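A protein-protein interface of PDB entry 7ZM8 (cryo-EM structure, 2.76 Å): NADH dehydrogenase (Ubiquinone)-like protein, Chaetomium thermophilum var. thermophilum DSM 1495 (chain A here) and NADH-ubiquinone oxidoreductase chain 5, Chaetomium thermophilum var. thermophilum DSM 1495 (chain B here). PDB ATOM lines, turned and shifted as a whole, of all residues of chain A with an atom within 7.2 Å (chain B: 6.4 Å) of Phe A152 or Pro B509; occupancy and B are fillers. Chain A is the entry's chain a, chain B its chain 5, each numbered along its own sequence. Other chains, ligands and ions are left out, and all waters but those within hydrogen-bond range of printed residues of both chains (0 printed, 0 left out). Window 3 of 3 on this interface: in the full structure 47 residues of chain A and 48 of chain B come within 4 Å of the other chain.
O of Phe A169 lies within hydrogen-bond range of N of Phe A152, at 3.2 Å.
The backbone carbonyl oxygen of Gly A155 is in hydrogen-bond range of the backbone NH of Ala A168.
A ring nitrogen (ND1) of His B508 sits close to the backbone NH (N) of Ile B510.
Of the 7 printed residues of chain B, 4 touch a printed residue of chain A.
Among the printed residues, 7 pairs touch across the chains.
Among the printed residues, Asp or Glu carboxylates within 4 Å of a Lys or Arg side-chain nitrogen of the other chain: Arg A150 with Glu B512.
Among the printed residues, pairs that only touch across the chains: Leu A160 with His B508, Arg A167 with Ile B510, Leu A160 with Pro B509, Ala A168 with Pro B509 and Phe A152 with Pro B509.
The guanidinium group of Arg A150 lies within salt-bridge range of the side-chain carboxylate of Glu B512.
O of Val A166 lies within hydrogen-bond range of NE2 of His B508 (3.4 Å).
Gly A154 touches none of the printed residues of chain B.
Printed residues of chain B within 4 Å of Val A166: His B508 (3.4 Å).
Ile B507 touches none of the printed residues of chain A.
Printed residues of chain A within 4 Å of Ile B510: Arg A167 (3.7 Å).
The nearest residue of chain A that does not touch Pro B509 is Leu A156 (4.5 Å).
The nearest printed residue of chain B that does not touch Ala A168 is Ile B510 (4.2 Å).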
ATOM      1  N   PRO A 149      26.896 -10.760 -35.963  1.00  0.00           N
ATOM      2  CA  PRO A 149      27.340 -10.561 -34.578  1.00  0.00           C
ATOM      3  C   PRO A 149      27.247 -11.845 -33.770  1.00  0.00           C
ATOM      4  O   PRO A 149      26.321 -12.639 -33.930  1.00  0.00           O
ATOM      5  CB  PRO A 149      26.383  -9.492 -34.047  1.00  0.00           C
ATOM      6  CG  PRO A 149      25.887  -8.791 -35.236  1.00  0.00           C
ATOM      7  CD  PRO A 149      25.920  -9.746 -36.388  1.00  0.00           C
ATOM      8  N   ARG A 150      28.227 -12.038 -32.892  1.00  0.00           N
ATOM      9  CA  ARG A 150      28.359 -13.295 -32.169  1.00  0.00           C
ATOM     10  C   ARG A 150      27.323 -13.364 -31.053  1.00  0.00           C
ATOM     11  O   ARG A 150      27.097 -12.385 -30.340  1.00  0.00           O
ATOM     12  CB  ARG A 150      29.776 -13.425 -31.617  1.00  0.00           C
ATOM     13  CG  ARG A 150      30.178 -14.833 -31.267  1.00  0.00           C
ATOM     14  CD  ARG A 150      31.660 -14.913 -30.993  1.00  0.00           C
ATOM     15  NE  ARG A 150      32.087 -13.863 -30.082  1.00  0.00           N
ATOM     16  CZ  ARG A 150      32.789 -14.084 -28.976  1.00  0.00           C
ATOM     17  NH1 ARG A 150      33.132 -13.076 -28.199  1.00  0.00           N
ATOM     18  NH2 ARG A 150      33.132 -15.317 -28.641  1.00  0.00           N
ATOM     19  N   GLU A 151      26.686 -14.520 -30.913  1.00  0.00           N
ATOM     20  CA  GLU A 151      25.489 -14.675 -30.096  1.00  0.00           C
ATOM     21  C   GLU A 151      25.810 -15.477 -28.842  1.00  0.00           C
ATOM     22  O   GLU A 151      26.451 -16.529 -28.920  1.00  0.00           O
ATOM     23  CB  GLU A 151      24.392 -15.371 -30.902  1.00  0.00           C
ATOM     24  CG  GLU A 151      23.164 -15.776 -30.117  1.00  0.00           C
ATOM     25  CD  GLU A 151      22.106 -14.698 -30.111  1.00  0.00           C
ATOM     26  OE1 GLU A 151      22.266 -13.708 -30.857  1.00  0.00           O
ATOM     27  OE2 GLU A 151      21.108 -14.850 -29.377  1.00  0.00           O
ATOM     28  N   PHE A 152      25.353 -14.989 -27.696  1.00  0.00           N
ATOM     29  CA  PHE A 152      25.683 -15.577 -26.407  1.00  0.00           C
ATOM     30  C   PHE A 152      24.458 -16.227 -25.782  1.00  0.00           C
ATOM     31  O   PHE A 152      23.326 -15.776 -25.988  1.00  0.00           O
ATOM     32  CB  PHE A 152      26.243 -14.521 -25.462  1.00  0.00           C
ATOM     33  CG  PHE A 152      27.678 -14.203 -25.708  1.00  0.00           C
ATOM     34  CD1 PHE A 152      28.675 -14.988 -25.164  1.00  0.00           C
ATOM     35  CD2 PHE A 152      28.035 -13.133 -26.510  1.00  0.00           C
ATOM     36  CE1 PHE A 152      29.999 -14.700 -25.391  1.00  0.00           C
ATOM     37  CE2 PHE A 152      29.356 -12.847 -26.743  1.00  0.00           C
ATOM     38  CZ  PHE A 152      30.339 -13.632 -26.180  1.00  0.00           C
ATOM     39  N   GLU A 153      24.695 -17.287 -25.016  1.00  0.00           N
ATOM     40  CA  GLU A 153      23.624 -17.995 -24.328  1.00  0.00           C
ATOM     41  C   GLU A 153      23.078 -17.119 -23.209  1.00  0.00           C
ATOM     42  O   GLU A 153      23.773 -16.855 -22.222  1.00  0.00           O
ATOM     43  CB  GLU A 153      24.141 -19.326 -23.788  1.00  0.00           C
ATOM     44  CG  GLU A 153      23.060 -20.253 -23.256  1.00  0.00           C
ATOM     45  CD  GLU A 153      22.671 -19.939 -21.826  1.00  0.00           C
ATOM     46  OE1 GLU A 153      23.525 -19.427 -21.074  1.00  0.00           O
ATOM     47  OE2 GLU A 153      21.507 -20.200 -21.456  1.00  0.00           O
ATOM     48  N   GLY A 154      21.843 -16.655 -23.364  1.00  0.00           N
ATOM     49  CA  GLY A 154      21.211 -15.834 -22.359  1.00  0.00           C
ATOM     50  C   GLY A 154      21.714 -14.412 -22.284  1.00  0.00           C
ATOM     51  O   GLY A 154      21.331 -13.687 -21.359  1.00  0.00           O
ATOM     52  N   GLY A 155      22.554 -13.985 -23.220  1.00  0.00           N
ATOM     53  CA  GLY A 155      23.132 -12.665 -23.165  1.00  0.00           C
ATOM     54  C   GLY A 155      24.132 -12.463 -22.054  1.00  0.00           C
ATOM     55  O   GLY A 155      24.588 -11.333 -21.859  1.00  0.00           O
ATOM     56  N   LEU A 156      24.483 -13.520 -21.318  1.00  0.00           N
ATOM     57  CA  LEU A 156      25.451 -13.444 -20.225  1.00  0.00           C
ATOM     58  C   LEU A 156      25.014 -12.424 -19.182  1.00  0.00           C
ATOM     59  O   LEU A 156      25.841 -11.812 -18.503  1.00  0.00           O
ATOM     60  CB  LEU A 156      26.850 -13.121 -20.749  1.00  0.00           C
ATOM     61  CG  LEU A 156      27.791 -14.270 -21.095  1.00  0.00           C
ATOM     62  CD1 LEU A 156      27.124 -15.239 -22.039  1.00  0.00           C
ATOM     63  CD2 LEU A 156      29.054 -13.723 -21.712  1.00  0.00           C
ATOM     64  N   LEU A 160      27.398 -10.285 -16.484  1.00  0.00           N
ATOM     65  CA  LEU A 160      27.711  -8.906 -16.819  1.00  0.00           C
ATOM     66  C   LEU A 160      27.046  -7.911 -15.881  1.00  0.00           C
ATOM     67  O   LEU A 160      27.102  -6.708 -16.136  1.00  0.00           O
ATOM     68  CB  LEU A 160      27.324  -8.619 -18.268  1.00  0.00           C
ATOM     69  CG  LEU A 160      28.326  -9.196 -19.268  1.00  0.00           C
ATOM     70  CD1 LEU A 160      27.667  -9.544 -20.590  1.00  0.00           C
ATOM     71  CD2 LEU A 160      29.473  -8.226 -19.473  1.00  0.00           C
ATOM     72  N   VAL A 166      24.169  -3.670 -18.785  1.00  0.00           N
ATOM     73  CA  VAL A 166      24.128  -3.975 -20.209  1.00  0.00           C
ATOM     74  C   VAL A 166      24.742  -5.345 -20.461  1.00  0.00           C
ATOM     75  O   VAL A 166      25.705  -5.748 -19.795  1.00  0.00           O
ATOM     76  CB  VAL A 166      24.842  -2.878 -21.014  1.00  0.00           C
ATOM     77  CG1 VAL A 166      26.324  -2.844 -20.682  1.00  0.00           C
ATOM     78  CG2 VAL A 166      24.624  -3.078 -22.506  1.00  0.00           C
ATOM     79  N   ARG A 167      24.174  -6.078 -21.411  1.00  0.00           N
ATOM     80  CA  ARG A 167      24.582  -7.440 -21.715  1.00  0.00           C
ATOM     81  C   ARG A 167      24.920  -7.565 -23.196  1.00  0.00           C
ATOM     82  O   ARG A 167      24.892  -6.592 -23.951  1.00  0.00           O
ATOM     83  CB  ARG A 167      23.485  -8.430 -21.329  1.00  0.00           C
ATOM     84  CG  ARG A 167      22.150  -8.143 -21.973  1.00  0.00           C
ATOM     85  CD  ARG A 167      21.469  -9.430 -22.389  1.00  0.00           C
ATOM     86  NE  ARG A 167      20.144  -9.196 -22.946  1.00  0.00           N
ATOM     87  CZ  ARG A 167      19.914  -8.878 -24.214  1.00  0.00           C
ATOM     88  NH1 ARG A 167      20.925  -8.756 -25.061  1.00  0.00           N
ATOM     89  NH2 ARG A 167      18.673  -8.681 -24.635  1.00  0.00           N
ATOM     90  N   ALA A 168      25.225  -8.792 -23.612  1.00  0.00           N
ATOM     91  CA  ALA A 168      25.684  -9.064 -24.960  1.00  0.00           C
ATOM     92  C   ALA A 168      24.516  -9.428 -25.875  1.00  0.00           C
ATOM     93  O   ALA A 168      23.348  -9.390 -25.487  1.00  0.00           O
ATOM     94  CB  ALA A 168      26.731 -10.171 -24.947  1.00  0.00           C
ATOM     95  N   PHE A 169      24.851  -9.795 -27.111  1.00  0.00           N
ATOM     96  CA  PHE A 169      23.851 -10.069 -28.135  1.00  0.00           C
ATOM     97  C   PHE A 169      23.044 -11.307 -27.770  1.00  0.00           C
ATOM     98  O   PHE A 169      23.600 -12.312 -27.322  1.00  0.00           O
ATOM     99  CB  PHE A 169      24.537 -10.257 -29.486  1.00  0.00           C
ATOM    100  CG  PHE A 169      23.684  -9.895 -30.662  1.00  0.00           C
ATOM    101  CD1 PHE A 169      23.152  -8.625 -30.779  1.00  0.00           C
ATOM    102  CD2 PHE A 169      23.423 -10.814 -31.655  1.00  0.00           C
ATOM    103  CE1 PHE A 169      22.370  -8.284 -31.865  1.00  0.00           C
ATOM    104  CE2 PHE A 169      22.646 -10.480 -32.744  1.00  0.00           C
ATOM    105  CZ  PHE A 169      22.116  -9.216 -32.848  1.00  0.00           C
ATOM    106  N   LEU A 170      21.725 -11.233 -27.958  1.00  0.00           N
ATOM    107  CA  LEU A 170      20.848 -12.352 -27.619  1.00  0.00           C
ATOM    108  C   LEU A 170      19.576 -12.248 -28.460  1.00  0.00           C
ATOM    109  O   LEU A 170      18.648 -11.525 -28.087  1.00  0.00           O
ATOM    110  CB  LEU A 170      20.536 -12.349 -26.129  1.00  0.00           C
ATOM    111  CG  LEU A 170      19.523 -13.361 -25.598  1.00  0.00           C
ATOM    112  CD1 LEU A 170      20.081 -14.770 -25.681  1.00  0.00           C
ATOM    113  CD2 LEU A 170      19.131 -13.014 -24.173  1.00  0.00           C
ATOM    114  N   CYS A 171      19.535 -12.994 -29.566  1.00  0.00           N
ATOM    115  CA  CYS A 171      18.346 -13.161 -30.415  1.00  0.00           C
ATOM    116  C   CYS A 171      17.557 -11.862 -30.582  1.00  0.00           C
ATOM    117  O   CYS A 171      16.369 -11.778 -30.262  1.00  0.00           O
ATOM    118  CB  CYS A 171      17.444 -14.268 -29.874  1.00  0.00           C
ATOM    119  SG  CYS A 171      18.234 -15.884 -29.708  1.00  0.00           S
ATOM    120  N   PHE B 506      39.401  -4.919 -18.812  1.00  0.00           N
ATOM    121  CA  PHE B 506      38.044  -5.390 -19.052  1.00  0.00           C
ATOM    122  C   PHE B 506      37.601  -5.014 -20.460  1.00  0.00           C
ATOM    123  O   PHE B 506      37.515  -3.830 -20.798  1.00  0.00           O
ATOM    124  CB  PHE B 506      37.088  -4.803 -18.017  1.00  0.00           C
ATOM    125  CG  PHE B 506      35.645  -5.066 -18.313  1.00  0.00           C
ATOM    126  CD1 PHE B 506      35.178  -6.358 -18.453  1.00  0.00           C
ATOM    127  CD2 PHE B 506      34.758  -4.023 -18.447  1.00  0.00           C
ATOM    128  CE1 PHE B 506      33.860  -6.600 -18.722  1.00  0.00           C
ATOM    129  CE2 PHE B 506      33.437  -4.263 -18.717  1.00  0.00           C
ATOM    130  CZ  PHE B 506      32.987  -5.554 -18.852  1.00  0.00           C
ATOM    131  N   ILE B 507      37.315  -6.024 -21.273  1.00  0.00           N
ATOM    132  CA  ILE B 507      36.678  -5.853 -22.572  1.00  0.00           C
ATOM    133  C   ILE B 507      35.240  -6.339 -22.473  1.00  0.00           C
ATOM    134  O   ILE B 507      34.978  -7.441 -21.979  1.00  0.00           O
ATOM    135  CB  ILE B 507      37.450  -6.588 -23.685  1.00  0.00           C
ATOM    136  CG1 ILE B 507      36.906  -6.198 -25.063  1.00  0.00           C
ATOM    137  CG2 ILE B 507      37.480  -8.099 -23.465  1.00  0.00           C
ATOM    138  CD1 ILE B 507      37.790  -6.616 -26.200  1.00  0.00           C
ATOM    139  N   HIS B 508      34.309  -5.506 -22.906  1.00  0.00           N
ATOM    140  CA  HIS B 508      32.904  -5.898 -22.860  1.00  0.00           C
ATOM    141  C   HIS B 508      32.556  -6.726 -24.089  1.00  0.00           C
ATOM    142  O   HIS B 508      32.919  -6.340 -25.205  1.00  0.00           O
ATOM    143  CB  HIS B 508      32.001  -4.681 -22.787  1.00  0.00           C
ATOM    144  CG  HIS B 508      30.630  -4.982 -22.269  1.00  0.00           C
ATOM    145  ND1 HIS B 508      29.680  -5.643 -23.016  1.00  0.00           N
ATOM    146  CD2 HIS B 508      30.055  -4.726 -21.072  1.00  0.00           C
ATOM    147  CE1 HIS B 508      28.578  -5.774 -22.302  1.00  0.00           C
ATOM    148  NE2 HIS B 508      28.778  -5.225 -21.119  1.00  0.00           N
ATOM    149  N   PRO B 509      31.899  -7.916 -23.945  1.00  0.00           N
ATOM    150  CA  PRO B 509      31.615  -8.792 -25.088  1.00  0.00           C
ATOM    151  C   PRO B 509      31.079  -8.064 -26.326  1.00  0.00           C
ATOM    152  O   PRO B 509      31.253  -8.568 -27.412  1.00  0.00           O
ATOM    153  CB  PRO B 509      30.587  -9.782 -24.539  1.00  0.00           C
ATOM    154  CG  PRO B 509      31.013  -9.968 -23.117  1.00  0.00           C
ATOM    155  CD  PRO B 509      31.439  -8.578 -22.698  1.00  0.00           C
ATOM    156  N   ILE B 510      30.442  -6.915 -26.130  1.00  0.00           N
ATOM    157  CA  ILE B 510      29.923  -6.106 -27.270  1.00  0.00           C
ATOM    158  C   ILE B 510      31.087  -5.575 -28.109  1.00  0.00           C
ATOM    159  O   ILE B 510      30.949  -5.541 -29.343  1.00  0.00           O
ATOM    160  CB  ILE B 510      28.974  -4.998 -26.769  1.00  0.00           C
ATOM    161  CG1 ILE B 510      29.671  -3.984 -25.863  1.00  0.00           C
ATOM    162  CG2 ILE B 510      27.758  -5.609 -26.091  1.00  0.00           C
ATOM    163  CD1 ILE B 510      28.753  -2.907 -25.336  1.00  0.00           C
ATOM    164  N   HIS B 511      32.193  -5.198 -27.469  1.00  0.00           N
ATOM    165  CA  HIS B 511      33.325  -4.554 -28.184  1.00  0.00           C
ATOM    166  C   HIS B 511      34.383  -5.548 -28.686  1.00  0.00           C
ATOM    167  O   HIS B 511      35.384  -5.076 -29.250  1.00  0.00           O
ATOM    168  CB  HIS B 511      33.932  -3.474 -27.291  1.00  0.00           C
ATOM    169  CG  HIS B 511      32.989  -2.398 -26.880  1.00  0.00           C
ATOM    170  ND1 HIS B 511      32.786  -2.067 -25.559  1.00  0.00           N
ATOM    171  CD2 HIS B 511      32.207  -1.573 -27.605  1.00  0.00           C
ATOM    172  CE1 HIS B 511      31.919  -1.082 -25.483  1.00  0.00           C
ATOM    173  NE2 HIS B 511      31.546  -0.761 -26.725  1.00  0.00           N
ATOM    174  N   GLU B 512      34.194  -6.852 -28.496  1.00  0.00           N
ATOM    175  CA  GLU B 512      35.242  -7.824 -28.896  1.00  0.00           C
ATOM    176  C   GLU B 512      35.337  -7.885 -30.427  1.00  0.00           C
ATOM    177  O   GLU B 512      34.286  -8.044 -31.077  1.00  0.00           O
ATOM    178  CB  GLU B 512      35.007  -9.165 -28.199  1.00  0.00           C
ATOM    179  CG  GLU B 512      34.569 -10.299 -29.107  1.00  0.00           C
ATOM    180  CD  GLU B 512      35.691 -11.055 -29.794  1.00  0.00           C
ATOM    181  OE1 GLU B 512      36.747 -11.237 -29.165  1.00  0.00           O
ATOM    182  OE2 GLU B 512      35.508 -11.442 -30.962  1.00  0.00           O
